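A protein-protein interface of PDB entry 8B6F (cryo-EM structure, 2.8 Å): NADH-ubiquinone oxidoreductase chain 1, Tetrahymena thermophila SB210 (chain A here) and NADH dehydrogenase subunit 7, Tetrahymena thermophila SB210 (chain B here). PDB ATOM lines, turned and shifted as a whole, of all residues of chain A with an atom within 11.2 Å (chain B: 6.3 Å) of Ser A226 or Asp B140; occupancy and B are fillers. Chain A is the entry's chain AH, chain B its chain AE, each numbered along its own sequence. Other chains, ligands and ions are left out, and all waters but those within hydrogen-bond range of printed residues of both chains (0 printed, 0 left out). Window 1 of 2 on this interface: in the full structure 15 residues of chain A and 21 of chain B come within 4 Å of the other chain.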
ATOM      1  N   TYR A 148     -33.422 -12.094 -14.596  1.00  0.00           N
ATOM      2  CA  TYR A 148     -32.298 -11.874 -13.691  1.00  0.00           C
ATOM      3  C   TYR A 148     -31.044 -12.579 -14.192  1.00  0.00           C
ATOM      4  O   TYR A 148     -29.945 -12.014 -14.143  1.00  0.00           O
ATOM      5  CB  TYR A 148     -32.657 -12.353 -12.286  1.00  0.00           C
ATOM      6  CG  TYR A 148     -33.832 -11.625 -11.681  1.00  0.00           C
ATOM      7  CD1 TYR A 148     -33.682 -10.354 -11.141  1.00  0.00           C
ATOM      8  CD2 TYR A 148     -35.091 -12.206 -11.647  1.00  0.00           C
ATOM      9  CE1 TYR A 148     -34.753  -9.681 -10.586  1.00  0.00           C
ATOM     10  CE2 TYR A 148     -36.169 -11.542 -11.094  1.00  0.00           C
ATOM     11  CZ  TYR A 148     -35.994 -10.280 -10.566  1.00  0.00           C
ATOM     12  OH  TYR A 148     -37.062  -9.616 -10.014  1.00  0.00           O
ATOM     13  N   MET A 151     -29.664 -10.586 -17.130  1.00  0.00           N
ATOM     14  CA  MET A 151     -28.958  -9.400 -16.656  1.00  0.00           C
ATOM     15  C   MET A 151     -27.613  -9.775 -16.047  1.00  0.00           C
ATOM     16  O   MET A 151     -26.624  -9.054 -16.214  1.00  0.00           O
ATOM     17  CB  MET A 151     -29.815  -8.640 -15.645  1.00  0.00           C
ATOM     18  CG  MET A 151     -31.002  -7.927 -16.272  1.00  0.00           C
ATOM     19  SD  MET A 151     -31.931  -6.912 -15.108  1.00  0.00           S
ATOM     20  CE  MET A 151     -32.583  -8.157 -13.999  1.00  0.00           C
ATOM     21  N   ALA A 152     -27.557 -10.906 -15.344  1.00  0.00           N
ATOM     22  CA  ALA A 152     -26.285 -11.388 -14.815  1.00  0.00           C
ATOM     23  C   ALA A 152     -25.307 -11.701 -15.939  1.00  0.00           C
ATOM     24  O   ALA A 152     -24.104 -11.443 -15.815  1.00  0.00           O
ATOM     25  CB  ALA A 152     -26.511 -12.625 -13.948  1.00  0.00           C
ATOM     26  N   ARG A 155     -23.924  -8.463 -17.146  1.00  0.00           N
ATOM     27  CA  ARG A 155     -22.920  -8.013 -16.189  1.00  0.00           C
ATOM     28  C   ARG A 155     -21.626  -8.794 -16.356  1.00  0.00           C
ATOM     29  O   ARG A 155     -20.532  -8.229 -16.257  1.00  0.00           O
ATOM     30  CB  ARG A 155     -23.441  -8.153 -14.761  1.00  0.00           C
ATOM     31  CG  ARG A 155     -24.555  -7.192 -14.412  1.00  0.00           C
ATOM     32  CD  ARG A 155     -24.931  -7.323 -12.953  1.00  0.00           C
ATOM     33  NE  ARG A 155     -25.935  -6.343 -12.562  1.00  0.00           N
ATOM     34  CZ  ARG A 155     -26.359  -6.167 -11.320  1.00  0.00           C
ATOM     35  NH1 ARG A 155     -25.885  -6.890 -10.319  1.00  0.00           N
ATOM     36  NH2 ARG A 155     -27.284  -5.245 -11.075  1.00  0.00           N
ATOM     37  N   ALA A 217     -15.714  -9.838  -4.207  1.00  0.00           N
ATOM     38  CA  ALA A 217     -16.103  -8.460  -3.953  1.00  0.00           C
ATOM     39  C   ALA A 217     -14.881  -7.555  -4.078  1.00  0.00           C
ATOM     40  O   ALA A 217     -13.771  -7.957  -3.714  1.00  0.00           O
ATOM     41  CB  ALA A 217     -16.722  -8.317  -2.563  1.00  0.00           C
ATOM     42  N   PRO A 218     -15.043  -6.326  -4.583  1.00  0.00           N
ATOM     43  CA  PRO A 218     -16.290  -5.677  -4.994  1.00  0.00           C
ATOM     44  C   PRO A 218     -16.676  -5.994  -6.432  1.00  0.00           C
ATOM     45  O   PRO A 218     -17.332  -5.193  -7.087  1.00  0.00           O
ATOM     46  CB  PRO A 218     -15.973  -4.177  -4.817  1.00  0.00           C
ATOM     47  CG  PRO A 218     -14.485  -4.081  -4.464  1.00  0.00           C
ATOM     48  CD  PRO A 218     -13.898  -5.423  -4.755  1.00  0.00           C
ATOM     49  N   ASP A 220     -18.232  -9.022  -7.522  1.00  0.00           N
ATOM     50  CA  ASP A 220     -19.171 -10.139  -7.607  1.00  0.00           C
ATOM     51  C   ASP A 220     -20.480  -9.700  -8.258  1.00  0.00           C
ATOM     52  O   ASP A 220     -21.569  -9.914  -7.731  1.00  0.00           O
ATOM     53  CB  ASP A 220     -19.410 -10.708  -6.213  1.00  0.00           C
ATOM     54  CG  ASP A 220     -20.272 -11.955  -6.230  1.00  0.00           C
ATOM     55  OD1 ASP A 220     -19.852 -12.962  -6.837  1.00  0.00           O
ATOM     56  OD2 ASP A 220     -21.366 -11.930  -5.629  1.00  0.00           O
ATOM     57  N   LEU A 221     -20.369  -9.077  -9.433  1.00  0.00           N
ATOM     58  CA  LEU A 221     -21.543  -8.524 -10.097  1.00  0.00           C
ATOM     59  C   LEU A 221     -22.379  -9.606 -10.767  1.00  0.00           C
ATOM     60  O   LEU A 221     -23.612  -9.553 -10.731  1.00  0.00           O
ATOM     61  CB  LEU A 221     -21.119  -7.470 -11.120  1.00  0.00           C
ATOM     62  CG  LEU A 221     -20.092  -6.446 -10.627  1.00  0.00           C
ATOM     63  CD1 LEU A 221     -19.790  -5.434 -11.715  1.00  0.00           C
ATOM     64  CD2 LEU A 221     -20.571  -5.748  -9.364  1.00  0.00           C
ATOM     65  N   ALA A 222     -21.728 -10.592 -11.386  1.00  0.00           N
ATOM     66  CA  ALA A 222     -22.468 -11.633 -12.092  1.00  0.00           C
ATOM     67  C   ALA A 222     -23.312 -12.461 -11.131  1.00  0.00           C
ATOM     68  O   ALA A 222     -24.459 -12.804 -11.439  1.00  0.00           O
ATOM     69  CB  ALA A 222     -21.502 -12.532 -12.863  1.00  0.00           C
ATOM     70  N   GLU A 223     -22.762 -12.792  -9.965  1.00  0.00           N
ATOM     71  CA  GLU A 223     -23.443 -13.620  -8.981  1.00  0.00           C
ATOM     72  C   GLU A 223     -24.046 -12.795  -7.849  1.00  0.00           C
ATOM     73  O   GLU A 223     -24.396 -13.352  -6.805  1.00  0.00           O
ATOM     74  CB  GLU A 223     -22.477 -14.667  -8.422  1.00  0.00           C
ATOM     75  CG  GLU A 223     -23.158 -15.808  -7.673  1.00  0.00           C
ATOM     76  CD  GLU A 223     -22.923 -15.761  -6.174  1.00  0.00           C
ATOM     77  OE1 GLU A 223     -21.813 -15.372  -5.752  1.00  0.00           O
ATOM     78  OE2 GLU A 223     -23.852 -16.111  -5.415  1.00  0.00           O
ATOM     79  N   ALA A 224     -24.164 -11.481  -8.033  1.00  0.00           N
ATOM     80  CA  ALA A 224     -24.740 -10.615  -7.011  1.00  0.00           C
ATOM     81  C   ALA A 224     -26.060 -11.182  -6.515  1.00  0.00           C
ATOM     82  O   ALA A 224     -27.025 -11.296  -7.275  1.00  0.00           O
ATOM     83  CB  ALA A 224     -24.942  -9.208  -7.574  1.00  0.00           C
ATOM     84  N   GLU A 225     -26.100 -11.531  -5.231  1.00  0.00           N
ATOM     85  CA  GLU A 225     -27.259 -12.186  -4.642  1.00  0.00           C
ATOM     86  C   GLU A 225     -28.296 -11.209  -4.107  1.00  0.00           C
ATOM     87  O   GLU A 225     -29.429 -11.623  -3.842  1.00  0.00           O
ATOM     88  CB  GLU A 225     -26.813 -13.128  -3.515  1.00  0.00           C
ATOM     89  CG  GLU A 225     -26.009 -12.456  -2.407  1.00  0.00           C
ATOM     90  CD  GLU A 225     -25.418 -13.456  -1.433  1.00  0.00           C
ATOM     91  OE1 GLU A 225     -25.791 -14.645  -1.501  1.00  0.00           O
ATOM     92  OE2 GLU A 225     -24.573 -13.056  -0.603  1.00  0.00           O
ATOM     93  N   SER A 226     -27.951  -9.933  -3.948  1.00  0.00           N
ATOM     94  CA  SER A 226     -28.907  -8.917  -3.524  1.00  0.00           C
ATOM     95  C   SER A 226     -29.504  -8.170  -4.708  1.00  0.00           C
ATOM     96  O   SER A 226     -30.725  -8.021  -4.797  1.00  0.00           O
ATOM     97  CB  SER A 226     -28.239  -7.927  -2.564  1.00  0.00           C
ATOM     98  OG  SER A 226     -27.182  -7.230  -3.201  1.00  0.00           O
ATOM     99  N   GLU A 227     -28.658  -7.690  -5.622  1.00  0.00           N
ATOM    100  CA  GLU A 227     -29.160  -7.021  -6.816  1.00  0.00           C
ATOM    101  C   GLU A 227     -29.957  -7.983  -7.688  1.00  0.00           C
ATOM    102  O   GLU A 227     -30.995  -7.613  -8.249  1.00  0.00           O
ATOM    103  CB  GLU A 227     -27.993  -6.419  -7.598  1.00  0.00           C
ATOM    104  CG  GLU A 227     -27.157  -5.434  -6.789  1.00  0.00           C
ATOM    105  CD  GLU A 227     -25.831  -5.112  -7.445  1.00  0.00           C
ATOM    106  OE1 GLU A 227     -25.622  -5.525  -8.603  1.00  0.00           O
ATOM    107  OE2 GLU A 227     -24.993  -4.447  -6.801  1.00  0.00           O
ATOM    108  N   LEU A 228     -29.484  -9.217  -7.813  1.00  0.00           N
ATOM    109  CA  LEU A 228     -30.172 -10.271  -8.539  1.00  0.00           C
ATOM    110  C   LEU A 228     -30.452 -11.422  -7.583  1.00  0.00           C
ATOM    111  O   LEU A 228     -29.822 -11.543  -6.530  1.00  0.00           O
ATOM    112  CB  LEU A 228     -29.339 -10.754  -9.732  1.00  0.00           C
ATOM    113  CG  LEU A 228     -28.876  -9.649 -10.685  1.00  0.00           C
ATOM    114  CD1 LEU A 228     -27.930 -10.204 -11.728  1.00  0.00           C
ATOM    115  CD2 LEU A 228     -30.062  -8.977 -11.352  1.00  0.00           C
ATOM    116  N   VAL A 229     -31.417 -12.265  -7.949  1.00  0.00           N
ATOM    117  CA  VAL A 229     -31.816 -13.354  -7.059  1.00  0.00           C
ATOM    118  C   VAL A 229     -30.605 -14.206  -6.700  1.00  0.00           C
ATOM    119  O   VAL A 229     -30.191 -14.273  -5.537  1.00  0.00           O
ATOM    120  CB  VAL A 229     -32.932 -14.197  -7.702  1.00  0.00           C
ATOM    121  CG1 VAL A 229     -33.260 -15.409  -6.840  1.00  0.00           C
ATOM    122  CG2 VAL A 229     -34.174 -13.347  -7.918  1.00  0.00           C
ATOM    123  N   THR A 230     -30.012 -14.861  -7.698  1.00  0.00           N
ATOM    124  CA  THR A 230     -28.800 -15.644  -7.484  1.00  0.00           C
ATOM    125  C   THR A 230     -27.730 -15.250  -8.490  1.00  0.00           C
ATOM    126  O   THR A 230     -26.533 -15.337  -8.197  1.00  0.00           O
ATOM    127  CB  THR A 230     -29.098 -17.143  -7.593  1.00  0.00           C
ATOM    128  OG1 THR A 230     -29.989 -17.536  -6.543  1.00  0.00           O
ATOM    129  CG2 THR A 230     -27.816 -17.964  -7.487  1.00  0.00           C
ATOM    130  N   GLY A 231     -28.149 -14.813  -9.679  1.00  0.00           N
ATOM    131  CA  GLY A 231     -27.237 -14.441 -10.741  1.00  0.00           C
ATOM    132  C   GLY A 231     -27.500 -15.262 -11.994  1.00  0.00           C
ATOM    133  O   GLY A 231     -28.652 -15.458 -12.394  1.00  0.00           O
ATOM    134  N   TYR A 232     -26.419 -15.742 -12.606  1.00  0.00           N
ATOM    135  CA  TYR A 232     -26.551 -16.540 -13.819  1.00  0.00           C
ATOM    136  C   TYR A 232     -27.089 -17.937 -13.539  1.00  0.00           C
ATOM    137  O   TYR A 232     -27.534 -18.612 -14.472  1.00  0.00           O
ATOM    138  CB  TYR A 232     -25.199 -16.637 -14.529  1.00  0.00           C
ATOM    139  CG  TYR A 232     -24.112 -17.287 -13.700  1.00  0.00           C
ATOM    140  CD1 TYR A 232     -23.920 -18.662 -13.726  1.00  0.00           C
ATOM    141  CD2 TYR A 232     -23.276 -16.525 -12.897  1.00  0.00           C
ATOM    142  CE1 TYR A 232     -22.929 -19.258 -12.972  1.00  0.00           C
ATOM    143  CE2 TYR A 232     -22.283 -17.111 -12.139  1.00  0.00           C
ATOM    144  CZ  TYR A 232     -22.114 -18.478 -12.181  1.00  0.00           C
ATOM    145  OH  TYR A 232     -21.124 -19.065 -11.428  1.00  0.00           O
ATOM    146  N   VAL A 234     -29.698 -18.734 -11.481  1.00  0.00           N
ATOM    147  CA  VAL A 234     -30.964 -18.597 -10.772  1.00  0.00           C
ATOM    148  C   VAL A 234     -31.918 -19.742 -11.079  1.00  0.00           C
ATOM    149  O   VAL A 234     -32.839 -19.998 -10.295  1.00  0.00           O
ATOM    150  CB  VAL A 234     -31.605 -17.239 -11.110  1.00  0.00           C
ATOM    151  CG1 VAL A 234     -32.072 -17.220 -12.541  1.00  0.00           C
ATOM    152  CG2 VAL A 234     -32.764 -16.948 -10.175  1.00  0.00           C
ATOM    153  N   PHE B  30     -39.782  -7.602  -9.445  1.00  0.00           N
ATOM    154  CA  PHE B  30     -38.898  -7.456  -8.297  1.00  0.00           C
ATOM    155  C   PHE B  30     -39.654  -7.860  -7.039  1.00  0.00           C
ATOM    156  O   PHE B  30     -40.582  -7.166  -6.616  1.00  0.00           O
ATOM    157  CB  PHE B  30     -38.395  -6.013  -8.208  1.00  0.00           C
ATOM    158  CG  PHE B  30     -37.431  -5.767  -7.086  1.00  0.00           C
ATOM    159  CD1 PHE B  30     -36.074  -5.971  -7.265  1.00  0.00           C
ATOM    160  CD2 PHE B  30     -37.882  -5.310  -5.859  1.00  0.00           C
ATOM    161  CE1 PHE B  30     -35.183  -5.737  -6.234  1.00  0.00           C
ATOM    162  CE2 PHE B  30     -36.997  -5.072  -4.824  1.00  0.00           C
ATOM    163  CZ  PHE B  30     -35.646  -5.285  -5.012  1.00  0.00           C
ATOM    164  N   HIS B  34     -37.555 -12.031  -3.215  1.00  0.00           N
ATOM    165  CA  HIS B  34     -36.320 -11.461  -3.714  1.00  0.00           C
ATOM    166  C   HIS B  34     -35.491 -11.057  -2.500  1.00  0.00           C
ATOM    167  O   HIS B  34     -36.035 -10.452  -1.560  1.00  0.00           O
ATOM    168  CB  HIS B  34     -36.577 -10.256  -4.620  1.00  0.00           C
ATOM    169  CG  HIS B  34     -35.375  -9.813  -5.394  1.00  0.00           C
ATOM    170  ND1 HIS B  34     -34.497  -8.858  -4.925  1.00  0.00           N
ATOM    171  CD2 HIS B  34     -34.908 -10.189  -6.607  1.00  0.00           C
ATOM    172  CE1 HIS B  34     -33.540  -8.669  -5.815  1.00  0.00           C
ATOM    173  NE2 HIS B  34     -33.765  -9.464  -6.845  1.00  0.00           N
ATOM    174  N   PRO B  35     -34.192 -11.374  -2.471  1.00  0.00           N
ATOM    175  CA  PRO B  35     -33.395 -11.010  -1.287  1.00  0.00           C
ATOM    176  C   PRO B  35     -33.420  -9.526  -0.970  1.00  0.00           C
ATOM    177  O   PRO B  35     -33.454  -9.151   0.208  1.00  0.00           O
ATOM    178  CB  PRO B  35     -31.986 -11.492  -1.660  1.00  0.00           C
ATOM    179  CG  PRO B  35     -32.212 -12.583  -2.637  1.00  0.00           C
ATOM    180  CD  PRO B  35     -33.408 -12.165  -3.434  1.00  0.00           C
ATOM    181  N   ALA B  36     -33.399  -8.664  -1.986  1.00  0.00           N
ATOM    182  CA  ALA B  36     -33.428  -7.228  -1.732  1.00  0.00           C
ATOM    183  C   ALA B  36     -34.790  -6.791  -1.204  1.00  0.00           C
ATOM    184  O   ALA B  36     -34.875  -6.025  -0.237  1.00  0.00           O
ATOM    185  CB  ALA B  36     -33.075  -6.463  -3.007  1.00  0.00           C
ATOM    186  N   ALA B  37     -35.865  -7.265  -1.826  1.00  0.00           N
ATOM    187  CA  ALA B  37     -37.200  -6.954  -1.341  1.00  0.00           C
ATOM    188  C   ALA B  37     -37.416  -7.572   0.034  1.00  0.00           C
ATOM    189  O   ALA B  37     -36.950  -8.680   0.315  1.00  0.00           O
ATOM    190  CB  ALA B  37     -38.256  -7.465  -2.319  1.00  0.00           C
ATOM    191  N   HIS B  38     -38.129  -6.848   0.897  1.00  0.00           N
ATOM    192  CA  HIS B  38     -38.358  -7.322   2.255  1.00  0.00           C
ATOM    193  C   HIS B  38     -39.229  -8.569   2.308  1.00  0.00           C
ATOM    194  O   HIS B  38     -39.278  -9.220   3.357  1.00  0.00           O
ATOM    195  CB  HIS B  38     -38.982  -6.212   3.097  1.00  0.00           C
ATOM    196  CG  HIS B  38     -38.022  -5.119   3.451  1.00  0.00           C
ATOM    197  ND1 HIS B  38     -37.242  -4.481   2.512  1.00  0.00           N
ATOM    198  CD2 HIS B  38     -37.708  -4.561   4.644  1.00  0.00           C
ATOM    199  CE1 HIS B  38     -36.493  -3.572   3.110  1.00  0.00           C
ATOM    200  NE2 HIS B  38     -36.756  -3.599   4.404  1.00  0.00           N
ATOM    201  N   ALA B 135     -27.733  -2.411   8.942  1.00  0.00           N
ATOM    202  CA  ALA B 135     -27.242  -3.737   8.589  1.00  0.00           C
ATOM    203  C   ALA B 135     -27.836  -4.218   7.273  1.00  0.00           C
ATOM    204  O   ALA B 135     -27.122  -4.756   6.419  1.00  0.00           O
ATOM    205  CB  ALA B 135     -27.568  -4.722   9.709  1.00  0.00           C
ATOM    206  N   CYS B 136     -29.146  -4.040   7.091  1.00  0.00           N
ATOM    207  CA  CYS B 136     -29.778  -4.464   5.848  1.00  0.00           C
ATOM    208  C   CYS B 136     -29.290  -3.630   4.671  1.00  0.00           C
ATOM    209  O   CYS B 136     -29.087  -4.154   3.571  1.00  0.00           O
ATOM    210  CB  CYS B 136     -31.297  -4.377   5.975  1.00  0.00           C
ATOM    211  SG  CYS B 136     -32.010  -5.590   7.112  1.00  0.00           S
ATOM    212  N   HIS B 137     -29.098  -2.328   4.885  1.00  0.00           N
ATOM    213  CA  HIS B 137     -28.568  -1.476   3.828  1.00  0.00           C
ATOM    214  C   HIS B 137     -27.174  -1.927   3.414  1.00  0.00           C
ATOM    215  O   HIS B 137     -26.869  -2.012   2.219  1.00  0.00           O
ATOM    216  CB  HIS B 137     -28.551  -0.022   4.301  1.00  0.00           C
ATOM    217  CG  HIS B 137     -28.281   0.967   3.212  1.00  0.00           C
ATOM    218  ND1 HIS B 137     -28.947   0.947   2.004  1.00  0.00           N
ATOM    219  CD2 HIS B 137     -27.425   2.013   3.151  1.00  0.00           C
ATOM    220  CE1 HIS B 137     -28.510   1.936   1.247  1.00  0.00           C
ATOM    221  NE2 HIS B 137     -27.586   2.599   1.919  1.00  0.00           N
ATOM    222  N   ALA B 138     -26.316  -2.226   4.388  1.00  0.00           N
ATOM    223  CA  ALA B 138     -24.975  -2.705   4.072  1.00  0.00           C
ATOM    224  C   ALA B 138     -25.024  -4.054   3.367  1.00  0.00           C
ATOM    225  O   ALA B 138     -24.250  -4.307   2.438  1.00  0.00           O
ATOM    226  CB  ALA B 138     -24.138  -2.797   5.348  1.00  0.00           C
ATOM    227  N   LEU B 139     -25.927  -4.937   3.799  1.00  0.00           N
ATOM    228  CA  LEU B 139     -26.064  -6.234   3.148  1.00  0.00           C
ATOM    229  C   LEU B 139     -26.501  -6.078   1.698  1.00  0.00           C
ATOM    230  O   LEU B 139     -25.982  -6.761   0.808  1.00  0.00           O
ATOM    231  CB  LEU B 139     -27.059  -7.102   3.918  1.00  0.00           C
ATOM    232  CG  LEU B 139     -27.158  -8.568   3.486  1.00  0.00           C
ATOM    233  CD1 LEU B 139     -25.848  -9.300   3.733  1.00  0.00           C
ATOM    234  CD2 LEU B 139     -28.298  -9.259   4.210  1.00  0.00           C
ATOM    235  N   ASP B 140     -27.456  -5.184   1.439  1.00  0.00           N
ATOM    236  CA  ASP B 140     -27.888  -4.944   0.067  1.00  0.00           C
ATOM    237  C   ASP B 140     -26.753  -4.385  -0.780  1.00  0.00           C
ATOM    238  O   ASP B 140     -26.565  -4.799  -1.930  1.00  0.00           O
ATOM    239  CB  ASP B 140     -29.077  -3.986   0.055  1.00  0.00           C
ATOM    240  CG  ASP B 140     -30.290  -4.556   0.759  1.00  0.00           C
ATOM    241  OD1 ASP B 140     -30.241  -5.733   1.171  1.00  0.00           O
ATOM    242  OD2 ASP B 140     -31.293  -3.825   0.902  1.00  0.00           O
ATOM    243  N   VAL B 141     -25.986  -3.441  -0.234  1.00  0.00           N
ATOM    244  CA  VAL B 141     -24.890  -2.857  -0.997  1.00  0.00           C
ATOM    245  C   VAL B 141     -23.799  -3.889  -1.251  1.00  0.00           C
ATOM    246  O   VAL B 141     -23.116  -3.835  -2.280  1.00  0.00           O
ATOM    247  CB  VAL B 141     -24.344  -1.612  -0.273  1.00  0.00           C
ATOM    248  CG1 VAL B 141     -23.092  -1.087  -0.962  1.00  0.00           C
ATOM    249  CG2 VAL B 141     -25.406  -0.528  -0.223  1.00  0.00           C
ATOM    250  N   GLY B 142     -23.609  -4.834  -0.334  1.00  0.00           N
ATOM    251  CA  GLY B 142     -22.640  -5.891  -0.544  1.00  0.00           C
ATOM    252  C   GLY B 142     -21.879  -6.307   0.698  1.00  0.00           C
ATOM    253  O   GLY B 142     -21.433  -7.452   0.793  1.00  0.00           O
ATOM    254  N   SER B 143     -21.726  -5.399   1.657  1.00  0.00           N
ATOM    255  CA  SER B 143     -20.997  -5.729   2.872  1.00  0.00           C
ATOM    256  C   SER B 143     -21.763  -6.775   3.673  1.00  0.00           C
ATOM    257  O   SER B 143     -22.977  -6.672   3.860  1.00  0.00           O
ATOM    258  CB  SER B 143     -20.773  -4.472   3.712  1.00  0.00           C
ATOM    259  OG  SER B 143     -20.007  -4.758   4.870  1.00  0.00           O
ATOM    260  N   ARG B 219     -21.053   4.463  -3.643  1.00  0.00           N
ATOM    261  CA  ARG B 219     -22.359   3.824  -3.748  1.00  0.00           C
ATOM    262  C   ARG B 219     -23.478   4.724  -3.236  1.00  0.00           C
ATOM    263  O   ARG B 219     -24.563   4.755  -3.825  1.00  0.00           O
ATOM    264  CB  ARG B 219     -22.358   2.498  -2.987  1.00  0.00           C
ATOM    265  CG  ARG B 219     -21.520   1.404  -3.635  1.00  0.00           C
ATOM    266  CD  ARG B 219     -22.239   0.728  -4.796  1.00  0.00           C
ATOM    267  NE  ARG B 219     -23.487   0.097  -4.381  1.00  0.00           N
ATOM    268  CZ  ARG B 219     -24.107  -0.861  -5.055  1.00  0.00           C
ATOM    269  NH1 ARG B 219     -23.606  -1.357  -6.172  1.00  0.00           N
ATOM    270  NH2 ARG B 219     -25.258  -1.340  -4.592  1.00  0.00           N
ATOM    271  N   ALA B 424     -28.702  -1.633  -9.228  1.00  0.00           N
ATOM    272  CA  ALA B 424     -27.850  -1.678  -8.046  1.00  0.00           C
ATOM    273  C   ALA B 424     -28.069  -0.466  -7.152  1.00  0.00           C
ATOM    274  O   ALA B 424     -27.892  -0.553  -5.932  1.00  0.00           O
ATOM    275  CB  ALA B 424     -26.385  -1.779  -8.460  1.00  0.00           C
ATOM    276  N   VAL B 427     -31.648  -1.064  -5.352  1.00  0.00           N
ATOM    277  CA  VAL B 427     -31.580  -1.949  -4.193  1.00  0.00           C
ATOM    278  C   VAL B 427     -30.999  -1.210  -2.997  1.00  0.00           C
ATOM    279  O   VAL B 427     -31.270  -1.569  -1.846  1.00  0.00           O
ATOM    280  CB  VAL B 427     -30.780  -3.224  -4.514  1.00  0.00           C
ATOM    281  CG1 VAL B 427     -31.473  -4.007  -5.612  1.00  0.00           C
ATOM    282  CG2 VAL B 427     -29.358  -2.889  -4.906  1.00  0.00           C
ATOM    283  N   ALA B 428     -30.182  -0.187  -3.239  1.00  0.00           N
ATOM    284  CA  ALA B 428     -29.710   0.649  -2.145  1.00  0.00           C
ATOM    285  C   ALA B 428     -30.795   1.616  -1.688  1.00  0.00           C
ATOM    286  O   ALA B 428     -30.922   1.891  -0.491  1.00  0.00           O
ATOM    287  CB  ALA B 428     -28.457   1.416  -2.569  1.00  0.00           C
ATOM    288  N   VAL B 430     -34.068   1.130  -1.725  1.00  0.00           N
ATOM    289  CA  VAL B 430     -35.077   0.430  -0.936  1.00  0.00           C
ATOM    290  C   VAL B 430     -34.595   0.257   0.497  1.00  0.00           C
ATOM    291  O   VAL B 430     -35.386   0.300   1.446  1.00  0.00           O
ATOM    292  CB  VAL B 430     -35.437  -0.922  -1.582  1.00  0.00           C
ATOM    293  CG1 VAL B 430     -36.070  -0.703  -2.947  1.00  0.00           C
ATOM    294  CG2 VAL B 430     -34.216  -1.813  -1.693  1.00  0.00           C
ATOM    295  N   GLY B 431     -33.291   0.038   0.677  1.00  0.00           N
ATOM    296  CA  GLY B 431     -32.744  -0.055   2.017  1.00  0.00           C
ATOM    297  C   GLY B 431     -32.609   1.281   2.715  1.00  0.00           C
ATOM    298  O   GLY B 431     -32.745   1.354   3.940  1.00  0.00           O
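Tyr A148 touches His B34 (CE1 to NE2, 3.9 Å).
Glu A225 touches Pro B35 (O to CG, 3.2 Å).
Ser A226 touches His B34 (O to CE1, 3.1 Å).
Ser A226 touches Ala B36 (O to CB, 3.3 Å).
NE2 of His B34 touches O of Glu A227, at 3.6 Å.
Ala B424 touches Glu A227 (CB to OE2, 3.4 Å).
Glu A227 touches Val B427.
Leu A228 touches His B34.
His B34 touches Val A229 (CD2 to CG2, 3.5 Å).
CG of Pro B35 touches O of Val A229 (3.9 Å).
Ser A226 touches just these residues of chain B: His B34, Ala B36 and Asp B140.
Pro B35 touches two residues of chain A.
Of chain A, only Ser A226 comes within 4 Å of Ala B36.
No residue of chain A comes within 4 Å of Ala B138.
No residue of chain A comes within 4 Å of Gly B142.
Printed residues of chain A within 4 Å of Val B427: Glu A227.
No residue of chain A comes within 4 Å of Ala B428.
No residue of chain A comes within 4 Å of Val B430.
No residue of chain A comes within 4 Å of Gly B431.
Of the printed residues of chain A, Ala B424 touches Glu A227.
Printed residues of chain B within 4 Å of Leu A228: His B34 (3.9 Å).
Ala A222 touches none of the printed residues of chain B.
The nearest printed residue of chain A that does not touch Arg B219 is Leu A221 (6.2 Å).
Printed residues of chain B that touch a printed residue of chain A: Phe B30, His B34, Pro B35, Ala B36, Asp B140, Arg B219, Ala B424 and Val B427.
Hydrophobic or aromatic side chains of chain B that line the printed part of chain A: His B34, Pro B35, Ala B36, Ala B424 and Val B427.
N of Ala B36 is in hydrogen-bond range of ND1 of His B34, at 3.1 Å.
The guanidinium group of Arg B219 sits at hydrogen-bond distance from the backbone carbonyl oxygen of Ala B424, 3.1 Å away.
The side-chain carboxylate (OE1) of Glu A227 lies within salt-bridge range of the guanidinium group (NH2) of Arg A155 (3.0 Å).
The side-chain hydroxyl (OG) of Ser A226 is in hydrogen-bond range of the backbone carbonyl oxygen (O) of Asp B140, 2.8 Å away.
OH of Tyr A148 sits close to N of Phe B30.
The guanidinium group (NH1) of Arg B219 lies within salt-bridge range of the side-chain carboxylate (OE2) of Glu A227 (3.4 Å).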
